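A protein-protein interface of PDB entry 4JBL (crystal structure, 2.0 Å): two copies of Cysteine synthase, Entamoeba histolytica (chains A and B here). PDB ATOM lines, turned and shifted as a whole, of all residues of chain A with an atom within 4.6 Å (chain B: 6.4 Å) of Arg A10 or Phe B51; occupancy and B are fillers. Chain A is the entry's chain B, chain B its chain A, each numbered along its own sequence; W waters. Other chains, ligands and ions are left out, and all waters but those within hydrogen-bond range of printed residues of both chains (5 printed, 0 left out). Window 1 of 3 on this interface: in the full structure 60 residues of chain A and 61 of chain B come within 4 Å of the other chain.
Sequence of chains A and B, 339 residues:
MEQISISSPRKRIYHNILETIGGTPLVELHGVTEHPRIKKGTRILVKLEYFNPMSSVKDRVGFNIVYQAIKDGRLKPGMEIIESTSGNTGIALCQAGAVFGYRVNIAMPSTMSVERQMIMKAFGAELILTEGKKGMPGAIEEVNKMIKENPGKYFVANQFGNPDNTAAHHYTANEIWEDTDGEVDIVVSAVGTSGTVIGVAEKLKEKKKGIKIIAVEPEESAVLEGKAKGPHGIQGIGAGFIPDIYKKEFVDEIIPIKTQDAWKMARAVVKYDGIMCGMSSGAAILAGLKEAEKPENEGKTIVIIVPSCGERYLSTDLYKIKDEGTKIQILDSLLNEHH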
ATOM      1  N   SER A   8     -17.866  -1.523 -10.880  1.00  0.00           N
ATOM      2  CA  SER A   8     -18.944  -1.535 -11.878  1.00  0.00           C
ATOM      3  C   SER A   8     -19.225  -0.122 -12.352  1.00  0.00           C
ATOM      4  O   SER A   8     -18.755   0.840 -11.706  1.00  0.00           O
ATOM      5  CB  SER A   8     -20.207  -2.116 -11.222  1.00  0.00           C
ATOM      6  OG  SER A   8     -19.928  -3.475 -10.984  1.00  0.00           O
ATOM      7  N   PRO A   9     -19.975   0.016 -13.450  1.00  0.00           N
ATOM      8  CA  PRO A   9     -20.304   1.368 -13.972  1.00  0.00           C
ATOM      9  C   PRO A   9     -21.006   2.190 -12.863  1.00  0.00           C
ATOM     10  O   PRO A   9     -21.712   1.622 -12.011  1.00  0.00           O
ATOM     11  CB  PRO A   9     -21.242   1.075 -15.141  1.00  0.00           C
ATOM     12  CG  PRO A   9     -20.757  -0.329 -15.641  1.00  0.00           C
ATOM     13  CD  PRO A   9     -20.521  -1.062 -14.328  1.00  0.00           C
ATOM     14  N   ARG A  10     -20.754   3.488 -12.808  1.00  0.00           N
ATOM     15  CA  ARG A  10     -21.455   4.352 -11.842  1.00  0.00           C
ATOM     16  C   ARG A  10     -22.954   4.591 -12.186  1.00  0.00           C
ATOM     17  O   ARG A  10     -23.739   4.906 -11.303  1.00  0.00           O
ATOM     18  CB  ARG A  10     -20.719   5.712 -11.802  1.00  0.00           C
ATOM     19  CG  ARG A  10     -19.370   5.633 -11.066  1.00  0.00           C
ATOM     20  CD  ARG A  10     -18.489   6.811 -11.489  1.00  0.00           C
ATOM     21  NE  ARG A  10     -17.249   6.823 -10.714  1.00  0.00           N
ATOM     22  CZ  ARG A  10     -16.972   7.685  -9.736  1.00  0.00           C
ATOM     23  NH1 ARG A  10     -17.890   8.613  -9.403  1.00  0.00           N
ATOM     24  NH2 ARG A  10     -15.798   7.593  -9.066  1.00  0.00           N
ATOM     25  N   LYS A  11     -23.321   4.412 -13.450  1.00  0.00           N
ATOM     26  CA  LYS A  11     -24.670   4.690 -14.001  1.00  0.00           C
ATOM     27  C   LYS A  11     -25.128   6.093 -13.618  1.00  0.00           C
ATOM     28  O   LYS A  11     -26.193   6.226 -13.071  1.00  0.00           O
ATOM     29  CB  LYS A  11     -25.765   3.757 -13.455  1.00  0.00           C
ATOM     30  CG  LYS A  11     -25.303   2.441 -12.899  1.00  0.00           C
ATOM     31  CD  LYS A  11     -25.510   1.387 -13.926  1.00  0.00           C
ATOM     32  CE  LYS A  11     -26.183   0.172 -13.308  1.00  0.00           C
ATOM     33  NZ  LYS A  11     -27.675   0.314 -13.300  1.00  0.00           N
ATOM     34  N   ARG A  12     -24.309   7.103 -13.868  1.00  0.00           N
ATOM     35  CA  ARG A  12     -24.630   8.514 -13.580  1.00  0.00           C
ATOM     36  C   ARG A  12     -23.877   9.227 -14.713  1.00  0.00           C
ATOM     37  O   ARG A  12     -22.797   8.751 -15.180  1.00  0.00           O
ATOM     38  CB  ARG A  12     -24.168   8.974 -12.118  1.00  0.00           C
ATOM     39  CG  ARG A  12     -24.774  10.379 -11.655  1.00  0.00           C
ATOM     40  CD  ARG A  12     -24.554  10.871 -10.213  1.00  0.00           C
ATOM     41  NE  ARG A  12     -24.903  12.302  -9.980  1.00  0.00           N
ATOM     42  CZ  ARG A  12     -24.519  13.073  -8.934  1.00  0.00           C
ATOM     43  NH1 ARG A  12     -23.690  12.645  -7.925  1.00  0.00           N
ATOM     44  NH2 ARG A  12     -24.958  14.342  -8.875  1.00  0.00           N
ATOM     45  N   TYR A  14     -22.453  12.904 -14.620  1.00  0.00           N
ATOM     46  CA  TYR A  14     -22.229  14.015 -13.707  1.00  0.00           C
ATOM     47  C   TYR A  14     -22.332  15.333 -14.495  1.00  0.00           C
ATOM     48  O   TYR A  14     -21.822  15.451 -15.629  1.00  0.00           O
ATOM     49  CB  TYR A  14     -20.846  13.855 -13.061  1.00  0.00           C
ATOM     50  CG  TYR A  14     -20.762  12.557 -12.270  1.00  0.00           C
ATOM     51  CD1 TYR A  14     -21.152  12.528 -10.926  1.00  0.00           C
ATOM     52  CD2 TYR A  14     -20.345  11.357 -12.900  1.00  0.00           C
ATOM     53  CE1 TYR A  14     -21.104  11.347 -10.191  1.00  0.00           C
ATOM     54  CE2 TYR A  14     -20.358  10.168 -12.216  1.00  0.00           C
ATOM     55  CZ  TYR A  14     -20.713  10.177 -10.856  1.00  0.00           C
ATOM     56  OH  TYR A  14     -20.640   8.986 -10.177  1.00  0.00           O
ATOM     57  N   ILE A  17     -17.641  18.671 -12.564  1.00  0.00           N
ATOM     58  CA  ILE A  17     -16.632  17.881 -11.793  1.00  0.00           C
ATOM     59  C   ILE A  17     -16.968  17.842 -10.293  1.00  0.00           C
ATOM     60  O   ILE A  17     -16.592  16.890  -9.586  1.00  0.00           O
ATOM     61  CB  ILE A  17     -15.197  18.457 -12.039  1.00  0.00           C
ATOM     62  CG1 ILE A  17     -14.068  17.462 -11.607  1.00  0.00           C
ATOM     63  CG2 ILE A  17     -15.049  19.803 -11.378  1.00  0.00           C
ATOM     64  CD1 ILE A  17     -14.118  16.130 -12.369  1.00  0.00           C
ATOM     65  N   THR A  20     -18.650  14.896  -8.763  1.00  0.00           N
ATOM     66  CA  THR A  20     -17.803  13.682  -8.585  1.00  0.00           C
ATOM     67  C   THR A  20     -17.075  13.694  -7.254  1.00  0.00           C
ATOM     68  O   THR A  20     -16.397  12.711  -6.920  1.00  0.00           O
ATOM     69  CB  THR A  20     -16.703  13.491  -9.652  1.00  0.00           C
ATOM     70  OG1 THR A  20     -15.700  14.518  -9.554  1.00  0.00           O
ATOM     71  CG2 THR A  20     -17.281  13.459 -11.090  1.00  0.00           C
ATOM     72  N   PHE A  51      -9.432   9.912  -3.834  1.00  0.00           N
ATOM     73  CA  PHE A  51     -10.240   9.597  -5.045  1.00  0.00           C
ATOM     74  C   PHE A  51     -11.105  10.827  -5.455  1.00  0.00           C
ATOM     75  O   PHE A  51     -11.736  10.814  -6.503  1.00  0.00           O
ATOM     76  CB  PHE A  51     -11.163   8.382  -4.798  1.00  0.00           C
ATOM     77  CG  PHE A  51     -10.503   7.063  -5.088  1.00  0.00           C
ATOM     78  CD1 PHE A  51      -9.376   6.675  -4.367  1.00  0.00           C
ATOM     79  CD2 PHE A  51     -11.016   6.236  -6.117  1.00  0.00           C
ATOM     80  CE1 PHE A  51      -8.728   5.464  -4.637  1.00  0.00           C
ATOM     81  CE2 PHE A  51     -10.392   5.013  -6.414  1.00  0.00           C
ATOM     82  CZ  PHE A  51      -9.273   4.622  -5.654  1.00  0.00           C
ATOM     83  N   PRO A  53     -11.859  14.528  -7.067  1.00  0.00           N
ATOM     84  CA  PRO A  53     -11.192  14.915  -8.356  1.00  0.00           C
ATOM     85  C   PRO A  53      -9.855  15.590  -8.219  1.00  0.00           C
ATOM     86  O   PRO A  53      -8.993  15.296  -9.052  1.00  0.00           O
ATOM     87  CB  PRO A  53     -12.213  15.844  -9.075  1.00  0.00           C
ATOM     88  CG  PRO A  53     -13.251  16.105  -8.026  1.00  0.00           C
ATOM     89  CD  PRO A  53     -13.258  14.984  -7.026  1.00  0.00           C
ATOM     90  N   SER B   7     -21.485  12.884  -4.839  1.00  0.00           N
ATOM     91  CA  SER B   7     -21.667  11.457  -5.053  1.00  0.00           C
ATOM     92  C   SER B   7     -22.137  10.783  -3.802  1.00  0.00           C
ATOM     93  O   SER B   7     -21.712  11.132  -2.677  1.00  0.00           O
ATOM     94  CB  SER B   7     -20.298  10.828  -5.401  1.00  0.00           C
ATOM     95  OG  SER B   7     -19.872  11.269  -6.664  1.00  0.00           O
ATOM     96  N   ARG B  10     -20.352   4.572  -1.943  1.00  0.00           N
ATOM     97  CA  ARG B  10     -20.220   3.417  -2.859  1.00  0.00           C
ATOM     98  C   ARG B  10     -20.944   2.168  -2.350  1.00  0.00           C
ATOM     99  O   ARG B  10     -21.205   1.243  -3.127  1.00  0.00           O
ATOM    100  CB  ARG B  10     -18.736   3.107  -3.076  1.00  0.00           C
ATOM    101  CG  ARG B  10     -18.020   4.086  -4.025  1.00  0.00           C
ATOM    102  CD  ARG B  10     -16.538   4.079  -3.723  1.00  0.00           C
ATOM    103  NE  ARG B  10     -15.904   5.058  -4.639  1.00  0.00           N
ATOM    104  CZ  ARG B  10     -15.174   4.671  -5.682  1.00  0.00           C
ATOM    105  NH1 ARG B  10     -15.035   3.389  -5.902  1.00  0.00           N
ATOM    106  NH2 ARG B  10     -14.610   5.562  -6.520  1.00  0.00           N
ATOM    107  N   THR B  20     -10.784  -1.102  -6.834  1.00  0.00           N
ATOM    108  CA  THR B  20     -11.284   0.277  -7.073  1.00  0.00           C
ATOM    109  C   THR B  20     -10.939   0.775  -8.510  1.00  0.00           C
ATOM    110  O   THR B  20     -11.242   1.922  -8.889  1.00  0.00           O
ATOM    111  CB  THR B  20     -10.677   1.327  -6.126  1.00  0.00           C
ATOM    112  OG1 THR B  20      -9.287   1.360  -6.386  1.00  0.00           O
ATOM    113  CG2 THR B  20     -10.913   0.951  -4.590  1.00  0.00           C
ATOM    114  N   GLY B  22     -11.383   1.058 -12.510  1.00  0.00           N
ATOM    115  CA  GLY B  22     -12.584   1.083 -13.319  1.00  0.00           C
ATOM    116  C   GLY B  22     -13.776   1.838 -12.719  1.00  0.00           C
ATOM    117  O   GLY B  22     -13.673   2.497 -11.686  1.00  0.00           O
ATOM    118  N   GLY B  23     -14.924   1.730 -13.391  1.00  0.00           N
ATOM    119  CA  GLY B  23     -16.144   2.468 -12.984  1.00  0.00           C
ATOM    120  C   GLY B  23     -15.823   3.945 -12.875  1.00  0.00           C
ATOM    121  O   GLY B  23     -16.158   4.630 -11.876  1.00  0.00           O
ATOM    122  N   THR B  24     -15.177   4.455 -13.902  1.00  0.00           N
ATOM    123  CA  THR B  24     -14.731   5.841 -13.854  1.00  0.00           C
ATOM    124  C   THR B  24     -15.873   6.780 -14.331  1.00  0.00           C
ATOM    125  O   THR B  24     -16.777   6.363 -15.099  1.00  0.00           O
ATOM    126  CB  THR B  24     -13.489   6.108 -14.715  1.00  0.00           C
ATOM    127  OG1 THR B  24     -13.828   5.749 -16.036  1.00  0.00           O
ATOM    128  CG2 THR B  24     -12.272   5.362 -14.212  1.00  0.00           C
ATOM    129  N   PRO B  25     -15.858   8.053 -13.838  1.00  0.00           N
ATOM    130  CA  PRO B  25     -17.040   8.903 -14.064  1.00  0.00           C
ATOM    131  C   PRO B  25     -17.103   9.586 -15.441  1.00  0.00           C
ATOM    132  O   PRO B  25     -16.045   9.974 -16.069  1.00  0.00           O
ATOM    133  CB  PRO B  25     -16.891   9.967 -12.983  1.00  0.00           C
ATOM    134  CG  PRO B  25     -15.366  10.082 -12.806  1.00  0.00           C
ATOM    135  CD  PRO B  25     -14.938   8.636 -12.844  1.00  0.00           C
ATOM    136  N   LEU B  26     -18.346   9.760 -15.898  1.00  0.00           N
ATOM    137  CA  LEU B  26     -18.583  10.384 -17.162  1.00  0.00           C
ATOM    138  C   LEU B  26     -19.173  11.753 -16.828  1.00  0.00           C
ATOM    139  O   LEU B  26     -20.262  11.849 -16.203  1.00  0.00           O
ATOM    140  CB  LEU B  26     -19.507   9.481 -18.002  1.00  0.00           C
ATOM    141  CG  LEU B  26     -19.736   9.926 -19.426  1.00  0.00           C
ATOM    142  CD1 LEU B  26     -18.371   9.754 -20.099  1.00  0.00           C
ATOM    143  CD2 LEU B  26     -20.751   8.939 -20.048  1.00  0.00           C
ATOM    144  N   VAL B  27     -18.496  12.819 -17.285  1.00  0.00           N
ATOM    145  CA  VAL B  27     -18.812  14.150 -16.788  1.00  0.00           C
ATOM    146  C   VAL B  27     -19.104  15.027 -18.009  1.00  0.00           C
ATOM    147  O   VAL B  27     -18.353  14.996 -18.990  1.00  0.00           O
ATOM    148  CB  VAL B  27     -17.649  14.780 -15.967  1.00  0.00           C
ATOM    149  CG1 VAL B  27     -18.050  16.183 -15.351  1.00  0.00           C
ATOM    150  CG2 VAL B  27     -17.217  13.848 -14.822  1.00  0.00           C
ATOM    151  N   LEU B  48     -13.300  10.154 -17.086  1.00  0.00           N
ATOM    152  CA  LEU B  48     -12.118  10.671 -16.447  1.00  0.00           C
ATOM    153  C   LEU B  48     -11.330   9.475 -15.892  1.00  0.00           C
ATOM    154  O   LEU B  48     -11.572   8.973 -14.806  1.00  0.00           O
ATOM    155  CB  LEU B  48     -12.576  11.678 -15.339  1.00  0.00           C
ATOM    156  CG  LEU B  48     -13.384  12.871 -15.863  1.00  0.00           C
ATOM    157  CD1 LEU B  48     -13.595  13.854 -14.644  1.00  0.00           C
ATOM    158  CD2 LEU B  48     -12.645  13.626 -16.989  1.00  0.00           C
ATOM    159  N   GLU B  49     -10.380   8.996 -16.658  1.00  0.00           N
ATOM    160  CA  GLU B  49      -9.653   7.792 -16.263  1.00  0.00           C
ATOM    161  C   GLU B  49      -8.640   8.052 -15.197  1.00  0.00           C
ATOM    162  O   GLU B  49      -8.022   7.105 -14.644  1.00  0.00           O
ATOM    163  CB  GLU B  49      -8.984   7.120 -17.486  1.00  0.00           C
ATOM    164  CG  GLU B  49     -10.031   6.552 -18.457  1.00  0.00           C
ATOM    165  CD  GLU B  49     -10.731   5.391 -17.821  1.00  0.00           C
ATOM    166  OE1 GLU B  49     -10.053   4.553 -17.206  1.00  0.00           O
ATOM    167  OE2 GLU B  49     -11.997   5.301 -17.842  1.00  0.00           O
ATOM    168  N   TYR B  50      -8.440   9.325 -14.877  1.00  0.00           N
ATOM    169  CA  TYR B  50      -7.614   9.623 -13.721  1.00  0.00           C
ATOM    170  C   TYR B  50      -8.362   9.355 -12.360  1.00  0.00           C
ATOM    171  O   TYR B  50      -7.736   9.399 -11.323  1.00  0.00           O
ATOM    172  CB  TYR B  50      -6.972  11.021 -13.799  1.00  0.00           C
ATOM    173  CG  TYR B  50      -7.929  12.186 -13.782  1.00  0.00           C
ATOM    174  CD1 TYR B  50      -8.438  12.708 -12.573  1.00  0.00           C
ATOM    175  CD2 TYR B  50      -8.326  12.807 -15.004  1.00  0.00           C
ATOM    176  CE1 TYR B  50      -9.278  13.823 -12.587  1.00  0.00           C
ATOM    177  CE2 TYR B  50      -9.192  13.894 -15.013  1.00  0.00           C
ATOM    178  CZ  TYR B  50      -9.620  14.391 -13.805  1.00  0.00           C
ATOM    179  OH  TYR B  50     -10.454  15.486 -13.864  1.00  0.00           O
ATOM    180  N   PHE B  51      -9.643   8.961 -12.368  1.00  0.00           N
ATOM    181  CA  PHE B  51     -10.250   8.445 -11.115  1.00  0.00           C
ATOM    182  C   PHE B  51      -9.756   7.040 -10.691  1.00  0.00           C
ATOM    183  O   PHE B  51      -9.995   6.610  -9.562  1.00  0.00           O
ATOM    184  CB  PHE B  51     -11.777   8.468 -11.214  1.00  0.00           C
ATOM    185  CG  PHE B  51     -12.333   9.837 -10.873  1.00  0.00           C
ATOM    186  CD1 PHE B  51     -12.033  10.949 -11.705  1.00  0.00           C
ATOM    187  CD2 PHE B  51     -13.168  10.009  -9.744  1.00  0.00           C
ATOM    188  CE1 PHE B  51     -12.532  12.238 -11.428  1.00  0.00           C
ATOM    189  CE2 PHE B  51     -13.641  11.292  -9.451  1.00  0.00           C
ATOM    190  CZ  PHE B  51     -13.338  12.394 -10.327  1.00  0.00           C
ATOM    191  N   ASN B  52      -9.039   6.338 -11.568  1.00  0.00           N
ATOM    192  CA  ASN B  52      -8.295   5.104 -11.154  1.00  0.00           C
ATOM    193  C   ASN B  52      -7.354   5.398  -9.966  1.00  0.00           C
ATOM    194  O   ASN B  52      -6.883   6.535  -9.837  1.00  0.00           O
ATOM    195  CB  ASN B  52      -7.519   4.578 -12.410  1.00  0.00           C
ATOM    196  CG  ASN B  52      -8.494   3.893 -13.366  1.00  0.00           C
ATOM    197  OD1 ASN B  52      -8.709   4.291 -14.550  1.00  0.00           O
ATOM    198  ND2 ASN B  52      -9.124   2.855 -12.846  1.00  0.00           N
ATOM    199  N   PRO B  53      -7.059   4.372  -9.116  1.00  0.00           N
ATOM    200  CA  PRO B  53      -6.303   4.615  -7.864  1.00  0.00           C
ATOM    201  C   PRO B  53      -4.920   5.231  -8.123  1.00  0.00           C
ATOM    202  O   PRO B  53      -4.397   5.989  -7.253  1.00  0.00           O
ATOM    203  CB  PRO B  53      -6.136   3.218  -7.268  1.00  0.00           C
ATOM    204  CG  PRO B  53      -6.598   2.157  -8.352  1.00  0.00           C
ATOM    205  CD  PRO B  53      -7.599   2.983  -9.181  1.00  0.00           C
ATOM    206  N   MET B  54      -4.305   4.957  -9.313  1.00  0.00           N
ATOM    207  CA  MET B  54      -3.029   5.644  -9.642  1.00  0.00           C
ATOM    208  C   MET B  54      -3.164   6.694 -10.761  1.00  0.00           C
ATOM    209  O   MET B  54      -2.184   7.031 -11.409  1.00  0.00           O
ATOM    210  CB  MET B  54      -1.805   4.666  -9.799  1.00  0.00           C
ATOM    211  CG  MET B  54      -1.204   4.237  -8.428  1.00  0.00           C
ATOM    212  SD  MET B  54      -0.737   5.558  -7.266  1.00  0.00           S
ATOM    213  CE  MET B  54       0.425   6.545  -8.223  1.00  0.00           C
ATOM    214  N   SER B  55      -4.376   7.204 -10.987  1.00  0.00           N
ATOM    215  CA  SER B  55      -4.614   8.414 -11.775  1.00  0.00           C
ATOM    216  C   SER B  55      -4.309   8.265 -13.263  1.00  0.00           C
ATOM    217  O   SER B  55      -4.100   9.257 -13.940  1.00  0.00           O
ATOM    218  CB  SER B  55      -3.863   9.625 -11.153  1.00  0.00           C
ATOM    219  OG  SER B  55      -4.147   9.573  -9.763  1.00  0.00           O
ATOM    220  N   SER B  56      -4.470   7.055 -13.813  1.00  0.00           N
ATOM    221  CA  SER B  56      -4.529   6.980 -15.284  1.00  0.00           C
ATOM    222  C   SER B  56      -5.221   5.723 -15.741  1.00  0.00           C
ATOM    223  O   SER B  56      -5.355   4.758 -14.980  1.00  0.00           O
ATOM    224  CB  SER B  56      -3.116   7.006 -15.934  1.00  0.00           C
ATOM    225  OG  SER B  56      -2.503   5.722 -15.936  1.00  0.00           O
ATOM    226  N   ASP B  59      -4.068   1.917 -15.173  1.00  0.00           N
ATOM    227  CA  ASP B  59      -4.356   1.009 -14.017  1.00  0.00           C
ATOM    228  C   ASP B  59      -5.098  -0.253 -14.502  1.00  0.00           C
ATOM    229  O   ASP B  59      -4.878  -1.349 -14.007  1.00  0.00           O
ATOM    230  CB  ASP B  59      -5.228   1.725 -12.926  1.00  0.00           C
ATOM    231  CG  ASP B  59      -4.434   2.763 -12.154  1.00  0.00           C
ATOM    232  OD1 ASP B  59      -3.294   3.080 -12.573  1.00  0.00           O
ATOM    233  OD2 ASP B  59      -4.911   3.189 -11.106  1.00  0.00           O
ATOM    234  N   GLU B 175     -19.003   0.541 -19.274  1.00  0.00           N
ATOM    235  CA  GLU B 175     -19.290   1.772 -18.478  1.00  0.00           C
ATOM    236  C   GLU B 175     -19.836   2.878 -19.370  1.00  0.00           C
ATOM    237  O   GLU B 175     -20.759   3.533 -18.991  1.00  0.00           O
ATOM    238  CB  GLU B 175     -17.995   2.218 -17.833  1.00  0.00           C
ATOM    239  CG  GLU B 175     -17.506   1.187 -16.827  1.00  0.00           C
ATOM    240  CD  GLU B 175     -16.077   1.449 -16.408  1.00  0.00           C
ATOM    241  OE1 GLU B 175     -15.639   2.623 -16.548  1.00  0.00           O
ATOM    242  OE2 GLU B 175     -15.384   0.470 -16.038  1.00  0.00           O
ATOM    243  N   ASP B 179     -23.544   4.069 -18.619  1.00  0.00           N
ATOM    244  CA  ASP B 179     -23.614   5.488 -18.135  1.00  0.00           C
ATOM    245  C   ASP B 179     -24.420   6.380 -19.117  1.00  0.00           C
ATOM    246  O   ASP B 179     -25.080   7.324 -18.669  1.00  0.00           O
ATOM    247  CB  ASP B 179     -22.222   6.101 -17.875  1.00  0.00           C
ATOM    248  CG  ASP B 179     -21.494   5.446 -16.688  1.00  0.00           C
ATOM    249  OD1 ASP B 179     -22.155   4.682 -15.921  1.00  0.00           O
ATOM    250  OD2 ASP B 179     -20.266   5.684 -16.446  1.00  0.00           O
HETATM  251  O   HOH W   1     -13.146   6.035  -8.956  1.00  0.00           O
HETATM  252  O   HOH W   2     -20.189   7.977 -14.726  1.00  0.00           O
HETATM  253  O   HOH W   3     -17.362  10.261  -7.275  1.00  0.00           O
HETATM  254  O   HOH W   4     -18.808   4.330 -14.888  1.00  0.00           O
HETATM  255  O   HOH W   5     -14.522   8.675  -6.626  1.00  0.00           O
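The backbone carbonyl oxygen (O) of Leu B26 is in hydrogen-bond range of the backbone NH (N) of Tyr A14, at 2.9 Å. The side-chain carboxylate (OD1) of Asp B179 is in hydrogen-bond range of the backbone NH (N) of Lys A11, at 2.7 Å. NE of Arg A10 is in hydrogen-bond range of O of Gly B23 (2.7 Å). The guanidinium group of Arg A10 lies close to the guanidinium group of Arg B10.
Arg A10 touches its own counterpart, Arg B10. Arg A10 touches Phe B51, and with the chains exchanged Phe A51 touches Arg B10. Phe A51 touches its own counterpart, Phe B51. Phe A51 touches Pro B53, and with the chains exchanged Pro A53 touches Phe B51. Of the 28 pairs that touch across the chains among the printed residues, 8 have their exchanged pair printed and touching as well.
Among the printed residues, merely in contact across the chains: Ile A17 with Leu B48 (3.3 Å), Thr A20 with Phe B51 (3.3 Å), Ser A8 with Gly B23 (3.3 Å), Phe A51 with Thr B20 (3.3 Å), Tyr A14 with Val B27 (3.5 Å), Phe A51 with Phe B51 (3.5 Å), Tyr A14 with Pro B25 (3.6 Å), Arg A10 with Asp B179 (3.6 Å), Arg A10 with Pro B25 (3.6 Å), Arg A10 with Phe B51 (3.6 Å), Phe A51 with Arg B10 (3.7 Å), Phe A51 with Pro B53 (3.7 Å), Arg A12 with Ser B7 (3.7 Å), Thr A20 with Ser B7 (3.7 Å), Tyr A14 with Ser B7 (3.7 Å), Thr A20 with Val B27 (3.8 Å), Ile A17 with Val B27 (3.8 Å), Pro A9 with Glu B175 (3.8 Å), Pro A9 with Asp B179 (3.8 Å), Arg A12 with Asp B179 (3.8 Å), Pro A53 with Phe B51 (3.8 Å), Pro A53 with Tyr B50 (3.8 Å), Arg A10 with Thr B24 (3.9 Å) and Thr A20 with Pro B25 (3.99 Å).
Of the 10 printed residues of chain A, 10 touch a printed residue of chain B. Printed residues of chain A that touch a printed residue of chain B: Ser A8, Pro A9, Arg A10, Lys A11, Arg A12, Tyr A14, Ile A17, Thr A20, Phe A51 and Pro A53. Hydrophobic or aromatic side chains of chain A that line the printed part of chain B: Pro A9, Tyr A14, Ile A17, Phe A51 and Pro A53. Among the printed residues, 28 pairs touch across the chains. Among the printed residues, no Asp or Glu carboxylate lies within 4 Å of a Lys or Arg side-chain nitrogen of the other chain.
Of chain B, only Arg B10 (3.5 Å), Gly B23 (2.7 Å), Thr B24 (3.9 Å), Pro B25 (3.6 Å), Phe B51 (3.6 Å) and Asp B179 (3.6 Å) come within 4 Å of Arg A10. Printed residues of chain A within 4 Å of Phe B51: Arg A10 (3.6 Å), Thr A20 (3.3 Å), Phe A51 (3.5 Å) and Pro A53 (3.8 Å). Of the printed residues of chain B, Phe A51 touches Arg B10 (3.7 Å), Thr B20 (3.3 Å), Phe B51 (3.5 Å) and Pro B53 (3.7 Å). Of the printed residues of chain A, Leu B26 touches Tyr A14. Printed residues of chain B within 4 Å of Pro A53: Tyr B50 (3.8 Å) and Phe B51 (3.8 Å). Printed residues of chain A within 4 Å of Ser B7: Arg A12 (3.7 Å), Tyr A14 (3.7 Å) and Thr A20 (3.7 Å). Asn B52 touches none of the printed residues of chain A. The nearest residue of chain B that does not touch Arg A10 is Ser B7 (4.3 Å). The nearest printed residue of chain B that does not touch Arg A12 is Leu B26 (4.1 Å).
N of Gly B23 sits at hydrogen-bond distance from OE2 of Glu B175 (3.0 Å). OG1 of Thr B24 lies within hydrogen-bond range of OE2 of Glu B49 (2.6 Å). O of Pro B25 lies within hydrogen-bond range of N of Leu B48 (2.9 Å). O of Ile A17 lies within hydrogen-bond range of OG1 of Thr A20, 2.5 Å away. OE1 of Glu B175 is in hydrogen-bond range of N of Thr B24, at 3.3 Å. NH1 of Arg A10 is in hydrogen-bond range of OH of Tyr A14.
Water W4 lies within hydrogen-bond range of the side-chain carboxylate of Asp B179, the backbone carbonyl oxygen of Thr B24 and the backbone NH of Arg A10. Water W3 lies within hydrogen-bond range of O of Thr A20 (2.7 Å), NH1 of Arg A10 (2.7 Å) and OG of Ser B7 (2.8 Å). Water W2 lies within hydrogen-bond range of the backbone carbonyl oxygen of Arg A12, the backbone NH of Leu B26 and the side-chain carboxylate of Asp B179. Water W1 lies within hydrogen-bond range of the guanidinium group (NH2) of Arg B10 (2.9 Å), the guanidinium group (NH2) of Arg A10 (3.1 Å) and the backbone carbonyl oxygen (O) of Phe B51 (3.3 Å). Water W5 lies within hydrogen-bond range of the guanidinium group (NH2) of Arg A10 (3.0 Å) and the guanidinium group (NH2) of Arg B10 (3.1 Å).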
